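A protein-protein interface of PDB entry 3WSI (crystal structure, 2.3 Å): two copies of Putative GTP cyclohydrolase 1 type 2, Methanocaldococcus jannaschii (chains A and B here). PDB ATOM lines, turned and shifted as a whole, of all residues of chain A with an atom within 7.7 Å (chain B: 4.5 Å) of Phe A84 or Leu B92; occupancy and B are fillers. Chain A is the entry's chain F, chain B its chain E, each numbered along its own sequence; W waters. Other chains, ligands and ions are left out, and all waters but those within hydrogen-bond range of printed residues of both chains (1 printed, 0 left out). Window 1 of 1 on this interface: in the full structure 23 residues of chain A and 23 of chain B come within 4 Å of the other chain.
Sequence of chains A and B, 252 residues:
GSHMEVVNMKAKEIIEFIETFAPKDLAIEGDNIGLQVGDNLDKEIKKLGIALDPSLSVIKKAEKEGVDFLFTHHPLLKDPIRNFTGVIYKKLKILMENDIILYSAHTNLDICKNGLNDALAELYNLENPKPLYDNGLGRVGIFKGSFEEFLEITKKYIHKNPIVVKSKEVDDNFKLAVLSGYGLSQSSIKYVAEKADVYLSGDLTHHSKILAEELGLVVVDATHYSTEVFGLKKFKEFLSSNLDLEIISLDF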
ATOM      1  N   LEU A  77      -9.832 -35.191  -4.013  1.00  0.00           N
ATOM      2  CA  LEU A  77     -11.096 -35.910  -4.065  1.00  0.00           C
ATOM      3  C   LEU A  77     -10.831 -37.385  -3.906  1.00  0.00           C
ATOM      4  O   LEU A  77      -9.886 -37.913  -4.505  1.00  0.00           O
ATOM      5  CB  LEU A  77     -11.822 -35.678  -5.390  1.00  0.00           C
ATOM      6  CG  LEU A  77     -12.284 -34.267  -5.765  1.00  0.00           C
ATOM      7  CD1 LEU A  77     -12.888 -34.347  -7.148  1.00  0.00           C
ATOM      8  CD2 LEU A  77     -13.263 -33.685  -4.749  1.00  0.00           C
ATOM      9  N   ILE A  81     -16.292 -36.933  -9.435  1.00  0.00           N
ATOM     10  CA  ILE A  81     -17.482 -36.107  -9.668  1.00  0.00           C
ATOM     11  C   ILE A  81     -17.629 -35.767 -11.144  1.00  0.00           C
ATOM     12  O   ILE A  81     -16.677 -35.882 -11.892  1.00  0.00           O
ATOM     13  CB  ILE A  81     -17.430 -34.773  -8.890  1.00  0.00           C
ATOM     14  CG1 ILE A  81     -16.265 -33.914  -9.394  1.00  0.00           C
ATOM     15  CG2 ILE A  81     -17.336 -35.011  -7.374  1.00  0.00           C
ATOM     16  CD1 ILE A  81     -16.133 -32.555  -8.696  1.00  0.00           C
ATOM     17  N   ARG A  82     -18.803 -35.294 -11.548  1.00  0.00           N
ATOM     18  CA  ARG A  82     -19.005 -34.864 -12.932  1.00  0.00           C
ATOM     19  C   ARG A  82     -19.775 -33.549 -12.996  1.00  0.00           C
ATOM     20  O   ARG A  82     -20.328 -33.210 -14.033  1.00  0.00           O
ATOM     21  CB  ARG A  82     -19.731 -35.940 -13.759  1.00  0.00           C
ATOM     22  CG  ARG A  82     -20.975 -36.526 -13.125  1.00  0.00           C
ATOM     23  CD  ARG A  82     -21.594 -37.618 -13.999  1.00  0.00           C
ATOM     24  NE  ARG A  82     -23.019 -37.759 -13.736  1.00  0.00           N
ATOM     25  CZ  ARG A  82     -23.844 -38.531 -14.438  1.00  0.00           C
ATOM     26  NH1 ARG A  82     -23.389 -39.266 -15.449  1.00  0.00           N
ATOM     27  NH2 ARG A  82     -25.135 -38.582 -14.124  1.00  0.00           N
ATOM     28  N   ASN A  83     -19.840 -32.837 -11.872  1.00  0.00           N
ATOM     29  CA  ASN A  83     -20.421 -31.494 -11.827  1.00  0.00           C
ATOM     30  C   ASN A  83     -19.553 -30.639 -10.929  1.00  0.00           C
ATOM     31  O   ASN A  83     -18.889 -31.163 -10.034  1.00  0.00           O
ATOM     32  CB  ASN A  83     -21.860 -31.500 -11.312  1.00  0.00           C
ATOM     33  CG  ASN A  83     -22.738 -32.490 -12.040  1.00  0.00           C
ATOM     34  OD1 ASN A  83     -22.789 -33.663 -11.672  1.00  0.00           O
ATOM     35  ND2 ASN A  83     -23.436 -32.029 -13.076  1.00  0.00           N
ATOM     36  N   PHE A  84     -19.547 -29.337 -11.170  1.00  0.00           N
ATOM     37  CA  PHE A  84     -18.604 -28.449 -10.500  1.00  0.00           C
ATOM     38  C   PHE A  84     -19.283 -27.227  -9.938  1.00  0.00           C
ATOM     39  O   PHE A  84     -19.439 -26.211 -10.614  1.00  0.00           O
ATOM     40  CB  PHE A  84     -17.484 -28.068 -11.471  1.00  0.00           C
ATOM     41  CG  PHE A  84     -16.818 -29.265 -12.062  1.00  0.00           C
ATOM     42  CD1 PHE A  84     -15.813 -29.923 -11.367  1.00  0.00           C
ATOM     43  CD2 PHE A  84     -17.234 -29.776 -13.265  1.00  0.00           C
ATOM     44  CE1 PHE A  84     -15.226 -31.055 -11.886  1.00  0.00           C
ATOM     45  CE2 PHE A  84     -16.646 -30.924 -13.793  1.00  0.00           C
ATOM     46  CZ  PHE A  84     -15.648 -31.560 -13.107  1.00  0.00           C
ATOM     47  N   THR A  85     -19.682 -27.347  -8.682  1.00  0.00           N
ATOM     48  CA  THR A  85     -20.441 -26.311  -8.022  1.00  0.00           C
ATOM     49  C   THR A  85     -19.900 -26.173  -6.597  1.00  0.00           C
ATOM     50  O   THR A  85     -19.038 -26.958  -6.175  1.00  0.00           O
ATOM     51  CB  THR A  85     -21.945 -26.651  -8.028  1.00  0.00           C
ATOM     52  OG1 THR A  85     -22.701 -25.484  -7.700  1.00  0.00           O
ATOM     53  CG2 THR A  85     -22.247 -27.735  -7.022  1.00  0.00           C
ATOM     54  N   GLY A  86     -20.378 -25.167  -5.872  1.00  0.00           N
ATOM     55  CA  GLY A  86     -20.038 -25.012  -4.464  1.00  0.00           C
ATOM     56  C   GLY A  86     -18.559 -25.021  -4.119  1.00  0.00           C
ATOM     57  O   GLY A  86     -17.745 -24.368  -4.766  1.00  0.00           O
ATOM     58  N   VAL A  87     -18.207 -25.793  -3.101  1.00  0.00           N
ATOM     59  CA  VAL A  87     -16.849 -25.741  -2.568  1.00  0.00           C
ATOM     60  C   VAL A  87     -15.802 -26.209  -3.584  1.00  0.00           C
ATOM     61  O   VAL A  87     -14.760 -25.560  -3.768  1.00  0.00           O
ATOM     62  CB  VAL A  87     -16.734 -26.579  -1.283  1.00  0.00           C
ATOM     63  CG1 VAL A  87     -15.296 -26.707  -0.862  1.00  0.00           C
ATOM     64  CG2 VAL A  87     -17.533 -25.928  -0.191  1.00  0.00           C
ATOM     65  N   ILE A  88     -16.072 -27.310  -4.267  1.00  0.00           N
ATOM     66  CA  ILE A  88     -15.063 -27.831  -5.191  1.00  0.00           C
ATOM     67  C   ILE A  88     -14.861 -26.842  -6.335  1.00  0.00           C
ATOM     68  O   ILE A  88     -13.751 -26.693  -6.829  1.00  0.00           O
ATOM     69  CB  ILE A  88     -15.420 -29.249  -5.729  1.00  0.00           C
ATOM     70  CG1 ILE A  88     -14.212 -29.850  -6.462  1.00  0.00           C
ATOM     71  CG2 ILE A  88     -16.656 -29.215  -6.629  1.00  0.00           C
ATOM     72  CD1 ILE A  88     -12.975 -30.033  -5.586  1.00  0.00           C
ATOM     73  N   TYR A  89     -15.917 -26.117  -6.696  1.00  0.00           N
ATOM     74  CA  TYR A  89     -15.821 -25.061  -7.697  1.00  0.00           C
ATOM     75  C   TYR A  89     -14.864 -23.941  -7.267  1.00  0.00           C
ATOM     76  O   TYR A  89     -14.009 -23.516  -8.044  1.00  0.00           O
ATOM     77  CB  TYR A  89     -17.201 -24.460  -7.985  1.00  0.00           C
ATOM     78  CG  TYR A  89     -17.174 -23.341  -9.029  1.00  0.00           C
ATOM     79  CD1 TYR A  89     -16.939 -22.014  -8.662  1.00  0.00           C
ATOM     80  CD2 TYR A  89     -17.348 -23.625 -10.382  1.00  0.00           C
ATOM     81  CE1 TYR A  89     -16.897 -20.997  -9.606  1.00  0.00           C
ATOM     82  CE2 TYR A  89     -17.301 -22.617 -11.339  1.00  0.00           C
ATOM     83  CZ  TYR A  89     -17.081 -21.301 -10.951  1.00  0.00           C
ATOM     84  OH  TYR A  89     -17.032 -20.288 -11.900  1.00  0.00           O
ATOM     85  N   LYS A  90     -15.029 -23.448  -6.044  1.00  0.00           N
ATOM     86  CA  LYS A  90     -14.178 -22.383  -5.517  1.00  0.00           C
ATOM     87  C   LYS A  90     -12.700 -22.819  -5.482  1.00  0.00           C
ATOM     88  O   LYS A  90     -11.796 -22.045  -5.789  1.00  0.00           O
ATOM     89  CB  LYS A  90     -14.639 -21.993  -4.104  1.00  0.00           C
ATOM     90  CG  LYS A  90     -16.006 -21.295  -4.043  1.00  0.00           C
ATOM     91  CD  LYS A  90     -16.421 -20.948  -2.598  1.00  0.00           C
ATOM     92  CE  LYS A  90     -17.656 -20.053  -2.573  1.00  0.00           C
ATOM     93  NZ  LYS A  90     -18.918 -20.748  -2.995  1.00  0.00           N
ATOM     94  N   LEU A  92     -11.177 -25.295  -7.304  1.00  0.00           N
ATOM     95  CA  LEU A  92     -10.605 -25.442  -8.630  1.00  0.00           C
ATOM     96  C   LEU A  92     -10.366 -24.085  -9.274  1.00  0.00           C
ATOM     97  O   LEU A  92      -9.334 -23.863  -9.908  1.00  0.00           O
ATOM     98  CB  LEU A  92     -11.497 -26.304  -9.520  1.00  0.00           C
ATOM     99  CG  LEU A  92     -11.520 -27.771  -9.084  1.00  0.00           C
ATOM    100  CD1 LEU A  92     -12.518 -28.576  -9.921  1.00  0.00           C
ATOM    101  CD2 LEU A  92     -10.130 -28.358  -9.203  1.00  0.00           C
ATOM    102  N   LYS A  93     -11.296 -23.160  -9.082  1.00  0.00           N
ATOM    103  CA  LYS A  93     -11.153 -21.854  -9.698  1.00  0.00           C
ATOM    104  C   LYS A  93      -9.880 -21.157  -9.197  1.00  0.00           C
ATOM    105  O   LYS A  93      -9.108 -20.621 -10.004  1.00  0.00           O
ATOM    106  CB  LYS A  93     -12.386 -20.996  -9.422  1.00  0.00           C
ATOM    107  CG  LYS A  93     -12.229 -19.515  -9.797  1.00  0.00           C
ATOM    108  CD  LYS A  93     -13.547 -18.749  -9.602  1.00  0.00           C
ATOM    109  CE  LYS A  93     -13.370 -17.246  -9.725  1.00  0.00           C
ATOM    110  NZ  LYS A  93     -13.051 -16.858 -11.117  1.00  0.00           N
ATOM    111  N   MET A  96      -6.908 -22.920 -10.710  1.00  0.00           N
ATOM    112  CA  MET A  96      -6.803 -22.855 -12.161  1.00  0.00           C
ATOM    113  C   MET A  96      -6.473 -21.484 -12.678  1.00  0.00           C
ATOM    114  O   MET A  96      -5.608 -21.346 -13.532  1.00  0.00           O
ATOM    115  CB  MET A  96      -8.085 -23.379 -12.802  1.00  0.00           C
ATOM    116  CG  MET A  96      -8.123 -24.894 -12.793  1.00  0.00           C
ATOM    117  SD  MET A  96      -9.702 -25.636 -13.205  1.00  0.00           S
ATOM    118  CE  MET A  96      -9.259 -27.370 -13.186  1.00  0.00           C
ATOM    119  N   GLU A  97      -7.110 -20.457 -12.144  1.00  0.00           N
ATOM    120  CA  GLU A  97      -6.837 -19.110 -12.627  1.00  0.00           C
ATOM    121  C   GLU A  97      -5.444 -18.630 -12.245  1.00  0.00           C
ATOM    122  O   GLU A  97      -4.906 -17.755 -12.900  1.00  0.00           O
ATOM    123  CB  GLU A  97      -7.893 -18.144 -12.126  1.00  0.00           C
ATOM    124  CG  GLU A  97      -7.815 -17.845 -10.658  1.00  0.00           C
ATOM    125  CD  GLU A  97      -9.002 -17.028 -10.192  1.00  0.00           C
ATOM    126  OE1 GLU A  97      -9.974 -16.879 -10.975  1.00  0.00           O
ATOM    127  OE2 GLU A  97      -8.973 -16.575  -9.028  1.00  0.00           O
ATOM    128  N   GLN B  36     -23.674 -27.936 -15.123  1.00  0.00           N
ATOM    129  CA  GLN B  36     -22.413 -28.656 -15.271  1.00  0.00           C
ATOM    130  C   GLN B  36     -21.322 -27.957 -14.477  1.00  0.00           C
ATOM    131  O   GLN B  36     -20.576 -28.590 -13.727  1.00  0.00           O
ATOM    132  CB  GLN B  36     -21.983 -28.731 -16.748  1.00  0.00           C
ATOM    133  CG  GLN B  36     -23.032 -29.203 -17.713  1.00  0.00           C
ATOM    134  CD  GLN B  36     -23.309 -30.702 -17.609  1.00  0.00           C
ATOM    135  OE1 GLN B  36     -22.437 -31.542 -17.864  1.00  0.00           O
ATOM    136  NE2 GLN B  36     -24.530 -31.038 -17.235  1.00  0.00           N
ATOM    137  N   VAL B  37     -21.216 -26.642 -14.696  1.00  0.00           N
ATOM    138  CA  VAL B  37     -20.208 -25.775 -14.082  1.00  0.00           C
ATOM    139  C   VAL B  37     -20.791 -24.411 -13.754  1.00  0.00           C
ATOM    140  O   VAL B  37     -21.322 -23.733 -14.650  1.00  0.00           O
ATOM    141  CB  VAL B  37     -18.988 -25.541 -15.012  1.00  0.00           C
ATOM    142  CG1 VAL B  37     -18.010 -24.567 -14.364  1.00  0.00           C
ATOM    143  CG2 VAL B  37     -18.309 -26.862 -15.373  1.00  0.00           C
ATOM    144  N   GLY B  38     -20.691 -24.002 -12.489  1.00  0.00           N
ATOM    145  CA  GLY B  38     -21.206 -22.710 -12.081  1.00  0.00           C
ATOM    146  C   GLY B  38     -21.425 -22.623 -10.592  1.00  0.00           C
ATOM    147  O   GLY B  38     -21.590 -23.640  -9.932  1.00  0.00           O
ATOM    148  N   LEU B  76     -20.967 -32.084 -20.056  1.00  0.00           N
ATOM    149  CA  LEU B  76     -19.513 -31.946 -20.081  1.00  0.00           C
ATOM    150  C   LEU B  76     -18.845 -33.286 -19.800  1.00  0.00           C
ATOM    151  O   LEU B  76     -17.907 -33.677 -20.497  1.00  0.00           O
ATOM    152  CB  LEU B  76     -19.046 -30.896 -19.078  1.00  0.00           C
ATOM    153  CG  LEU B  76     -17.541 -30.642 -19.014  1.00  0.00           C
ATOM    154  CD1 LEU B  76     -17.055 -29.996 -20.310  1.00  0.00           C
ATOM    155  CD2 LEU B  76     -17.222 -29.733 -17.797  1.00  0.00           C
ATOM    156  N   LEU B  77     -19.321 -33.990 -18.783  1.00  0.00           N
ATOM    157  CA  LEU B  77     -18.736 -35.283 -18.441  1.00  0.00           C
ATOM    158  C   LEU B  77     -19.868 -36.276 -18.286  1.00  0.00           C
ATOM    159  O   LEU B  77     -20.889 -35.952 -17.669  1.00  0.00           O
ATOM    160  CB  LEU B  77     -17.906 -35.195 -17.146  1.00  0.00           C
ATOM    161  CG  LEU B  77     -16.647 -34.316 -17.101  1.00  0.00           C
ATOM    162  CD1 LEU B  77     -16.129 -34.216 -15.692  1.00  0.00           C
ATOM    163  CD2 LEU B  77     -15.552 -34.904 -17.955  1.00  0.00           C
ATOM    164  N   PHE B  84      -7.732 -33.493 -12.427  1.00  0.00           N
ATOM    165  CA  PHE B  84      -8.085 -32.440 -13.372  1.00  0.00           C
ATOM    166  C   PHE B  84      -6.888 -31.953 -14.110  1.00  0.00           C
ATOM    167  O   PHE B  84      -6.204 -31.030 -13.660  1.00  0.00           O
ATOM    168  CB  PHE B  84      -8.781 -31.309 -12.633  1.00  0.00           C
ATOM    169  CG  PHE B  84      -9.957 -31.786 -11.866  1.00  0.00           C
ATOM    170  CD1 PHE B  84     -11.176 -31.935 -12.497  1.00  0.00           C
ATOM    171  CD2 PHE B  84      -9.824 -32.194 -10.546  1.00  0.00           C
ATOM    172  CE1 PHE B  84     -12.265 -32.429 -11.803  1.00  0.00           C
ATOM    173  CE2 PHE B  84     -10.895 -32.681  -9.855  1.00  0.00           C
ATOM    174  CZ  PHE B  84     -12.118 -32.805 -10.475  1.00  0.00           C
ATOM    175  N   ILE B  88      -9.550 -31.504 -19.863  1.00  0.00           N
ATOM    176  CA  ILE B  88     -10.594 -31.087 -18.937  1.00  0.00           C
ATOM    177  C   ILE B  88     -10.057 -29.924 -18.081  1.00  0.00           C
ATOM    178  O   ILE B  88     -10.800 -28.999 -17.741  1.00  0.00           O
ATOM    179  CB  ILE B  88     -11.105 -32.277 -18.056  1.00  0.00           C
ATOM    180  CG1 ILE B  88     -12.411 -31.891 -17.378  1.00  0.00           C
ATOM    181  CG2 ILE B  88     -10.028 -32.768 -17.065  1.00  0.00           C
ATOM    182  CD1 ILE B  88     -13.514 -31.568 -18.383  1.00  0.00           C
ATOM    183  N   TYR B  89      -8.756 -29.929 -17.805  1.00  0.00           N
ATOM    184  CA  TYR B  89      -8.144 -28.804 -17.093  1.00  0.00           C
ATOM    185  C   TYR B  89      -8.282 -27.505 -17.900  1.00  0.00           C
ATOM    186  O   TYR B  89      -8.670 -26.469 -17.346  1.00  0.00           O
ATOM    187  CB  TYR B  89      -6.660 -29.058 -16.784  1.00  0.00           C
ATOM    188  CG  TYR B  89      -5.983 -27.866 -16.102  1.00  0.00           C
ATOM    189  CD1 TYR B  89      -5.429 -26.819 -16.858  1.00  0.00           C
ATOM    190  CD2 TYR B  89      -5.899 -27.781 -14.705  1.00  0.00           C
ATOM    191  CE1 TYR B  89      -4.818 -25.727 -16.238  1.00  0.00           C
ATOM    192  CE2 TYR B  89      -5.291 -26.696 -14.075  1.00  0.00           C
ATOM    193  CZ  TYR B  89      -4.757 -25.675 -14.835  1.00  0.00           C
ATOM    194  OH  TYR B  89      -4.160 -24.599 -14.201  1.00  0.00           O
ATOM    195  N   LYS B  90      -7.948 -27.562 -19.190  1.00  0.00           N
ATOM    196  CA  LYS B  90      -8.030 -26.385 -20.055  1.00  0.00           C
ATOM    197  C   LYS B  90      -9.446 -25.861 -20.136  1.00  0.00           C
ATOM    198  O   LYS B  90      -9.653 -24.659 -20.175  1.00  0.00           O
ATOM    199  CB  LYS B  90      -7.487 -26.674 -21.462  1.00  0.00           C
ATOM    200  CG  LYS B  90      -5.968 -26.850 -21.493  1.00  0.00           C
ATOM    201  CD  LYS B  90      -5.437 -27.085 -22.909  1.00  0.00           C
ATOM    202  CE  LYS B  90      -4.778 -28.460 -23.047  1.00  0.00           C
ATOM    203  NZ  LYS B  90      -3.341 -28.408 -22.623  1.00  0.00           N
ATOM    204  N   LYS B  91     -10.418 -26.760 -20.171  1.00  0.00           N
ATOM    205  CA  LYS B  91     -11.822 -26.365 -20.268  1.00  0.00           C
ATOM    206  C   LYS B  91     -12.361 -25.684 -19.006  1.00  0.00           C
ATOM    207  O   LYS B  91     -12.981 -24.618 -19.088  1.00  0.00           O
ATOM    208  CB  LYS B  91     -12.679 -27.595 -20.630  1.00  0.00           C
ATOM    209  CG  LYS B  91     -12.392 -28.116 -22.029  1.00  0.00           C
ATOM    210  CD  LYS B  91     -12.930 -29.521 -22.254  1.00  0.00           C
ATOM    211  CE  LYS B  91     -14.124 -29.496 -23.124  1.00  0.00           C
ATOM    212  NZ  LYS B  91     -14.579 -30.840 -23.575  1.00  0.00           N
ATOM    213  N   LEU B  92     -12.133 -26.304 -17.848  1.00  0.00           N
ATOM    214  CA  LEU B  92     -12.594 -25.776 -16.558  1.00  0.00           C
ATOM    215  C   LEU B  92     -11.887 -24.464 -16.233  1.00  0.00           C
ATOM    216  O   LEU B  92     -12.477 -23.553 -15.628  1.00  0.00           O
ATOM    217  CB  LEU B  92     -12.368 -26.800 -15.437  1.00  0.00           C
ATOM    218  CG  LEU B  92     -13.251 -28.026 -15.626  1.00  0.00           C
ATOM    219  CD1 LEU B  92     -12.991 -29.109 -14.585  1.00  0.00           C
ATOM    220  CD2 LEU B  92     -14.697 -27.590 -15.617  1.00  0.00           C
ATOM    221  N   LYS B  93     -10.611 -24.376 -16.599  1.00  0.00           N
ATOM    222  CA  LYS B  93      -9.868 -23.160 -16.302  1.00  0.00           C
ATOM    223  C   LYS B  93     -10.517 -21.975 -17.010  1.00  0.00           C
ATOM    224  O   LYS B  93     -10.690 -20.922 -16.417  1.00  0.00           O
ATOM    225  CB  LYS B  93      -8.394 -23.291 -16.697  1.00  0.00           C
ATOM    226  CG  LYS B  93      -7.617 -21.959 -16.670  1.00  0.00           C
ATOM    227  CD  LYS B  93      -6.135 -22.204 -16.912  1.00  0.00           C
ATOM    228  CE  LYS B  93      -5.346 -20.917 -17.176  1.00  0.00           C
ATOM    229  NZ  LYS B  93      -5.238 -20.038 -16.003  1.00  0.00           N
ATOM    230  N   ILE B  94     -10.910 -22.163 -18.268  1.00  0.00           N
ATOM    231  CA  ILE B  94     -11.565 -21.092 -19.003  1.00  0.00           C
ATOM    232  C   ILE B  94     -12.938 -20.746 -18.411  1.00  0.00           C
ATOM    233  O   ILE B  94     -13.248 -19.575 -18.211  1.00  0.00           O
ATOM    234  CB  ILE B  94     -11.724 -21.446 -20.503  1.00  0.00           C
ATOM    235  CG1 ILE B  94     -10.357 -21.496 -21.193  1.00  0.00           C
ATOM    236  CG2 ILE B  94     -12.600 -20.425 -21.203  1.00  0.00           C
ATOM    237  CD1 ILE B  94     -10.387 -22.217 -22.537  1.00  0.00           C
ATOM    238  N   LEU B  95     -13.752 -21.758 -18.123  1.00  0.00           N
ATOM    239  CA  LEU B  95     -15.079 -21.505 -17.568  1.00  0.00           C
ATOM    240  C   LEU B  95     -14.983 -20.827 -16.210  1.00  0.00           C
ATOM    241  O   LEU B  95     -15.756 -19.904 -15.898  1.00  0.00           O
ATOM    242  CB  LEU B  95     -15.892 -22.792 -17.435  1.00  0.00           C
ATOM    243  CG  LEU B  95     -16.208 -23.529 -18.732  1.00  0.00           C
ATOM    244  CD1 LEU B  95     -16.897 -24.872 -18.451  1.00  0.00           C
ATOM    245  CD2 LEU B  95     -17.032 -22.651 -19.674  1.00  0.00           C
ATOM    246  N   MET B  96     -14.029 -21.274 -15.400  1.00  0.00           N
ATOM    247  CA  MET B  96     -13.988 -20.799 -14.028  1.00  0.00           C
ATOM    248  C   MET B  96     -13.378 -19.406 -13.911  1.00  0.00           C
ATOM    249  O   MET B  96     -13.900 -18.564 -13.189  1.00  0.00           O
ATOM    250  CB  MET B  96     -13.256 -21.810 -13.147  1.00  0.00           C
ATOM    251  CG  MET B  96     -14.146 -23.014 -12.805  1.00  0.00           C
ATOM    252  SD  MET B  96     -13.233 -24.388 -12.080  1.00  0.00           S
ATOM    253  CE  MET B  96     -14.576 -25.524 -11.741  1.00  0.00           C
HETATM  254  O   HOH W   1     -18.584 -20.757 -14.035  1.00  0.00           O
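N of Gly B38 sits at hydrogen-bond distance from O of Phe A84 (3.2 Å).
OG1 of Thr A85 sits at hydrogen-bond distance from O of Gly B38 (3.1 Å).
The backbone carbonyl oxygen (O) of Gln B36 sits at hydrogen-bond distance from the backbone NH (N) of Phe A84 (2.9 Å).
NZ of Lys A93 sits at hydrogen-bond distance from O of Met B96, 2.8 Å away.
The side-chain amino group (NZ) of Lys B93 is in hydrogen-bond range of the backbone carbonyl oxygen (O) of Met A96, 2.8 Å away.
Phe A84 touches seven residues of chain B.
Printed residues of chain B within 4 Å of Thr A85: Gly B38 (3.1 Å).
Ile A88 touches none of the printed residues of chain B.
Of the printed residues of chain A, Gly B38 touches Phe A84, Thr A85 and Tyr A89.
Of the printed residues of chain A, Phe B84 touches Leu A77 (3.7 Å) and Phe A84 (3.3 Å).
Of chain A, only Phe A84 and Met A96 come within 4 Å of Leu B92.
Of the printed residues of chain A, Met B96 touches Phe A84, Tyr A89, Leu A92, Lys A93 and Met A96.
The nearest printed residue of chain A that does not touch Gly B38 is Gly A86 (4.5 Å).
Among the printed residues, pairs that only touch across the chains: Leu A77 with Phe B84 (3.7 Å), Arg A82 with Leu B77 (3.9 Å), Asn A83 with Gln B36 (3.5 Å), Phe A84 with Val B37 (3.6 Å), Phe A84 with Leu B77 (3.7 Å), Phe A84 with Phe B84 (3.3 Å), Phe A84 with Leu B92 (3.9 Å), Phe A84 with Met B96 (3.9 Å), Tyr A89 with Val B37 (3.7 Å), Tyr A89 with Gly B38 (3.8 Å), Tyr A89 with Met B96 (3.5 Å), Leu A92 with Met B96 (3.6 Å), Met A96 with Tyr B89 (3.6 Å), Met A96 with Leu B92 (3.7 Å), Met A96 with Met B96 (3.9 Å) and Glu A97 with Lys B93 (3.8 Å).
Phe A84 touches Leu B92, but with the chains exchanged Leu A92 does not touch Phe B84 (4.1 Å).
Phe A84 touches Met B96, but with the chains exchanged Met A96 does not touch Phe B84 (4.01 Å).
Tyr A89 touches Met B96, and with the chains exchanged Met A96 touches Tyr B89.
Leu A92 touches Met B96, and with the chains exchanged Met A96 touches Leu B92.
Positions printed for both chains: 77, 84, 88, 89, 90, 92, 93 and 96.
Of the 21 pairs that touch across the chains among the printed residues, 10 have their exchanged pair printed and touching as well.
The backbone NH (N) of Leu B76 lies within hydrogen-bond range of the side-chain amide oxygen (OE1) of Gln B36, 2.7 Å away.
NZ of Lys A93 lies within salt-bridge range of OE1 of Glu A97.
Printed residues of chain A that touch a printed residue of chain B: Leu A77, Arg A82, Asn A83, Phe A84, Thr A85, Tyr A89, Leu A92, Lys A93, Met A96 and Glu A97.
Hydrophobic or aromatic side chains of chain A that line the printed part of chain B: Leu A77, Phe A84, Tyr A89, Leu A92 and Met A96.
Among the printed residues, 21 pairs touch across the chains.
Among the printed residues, no Asp or Glu carboxylate lies within 4 Å of a Lys or Arg side-chain nitrogen of the other chain.
Water W1 bridges the side-chain hydroxyl (OH) of Tyr A89 and the backbone carbonyl oxygen (O) of Leu B95.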
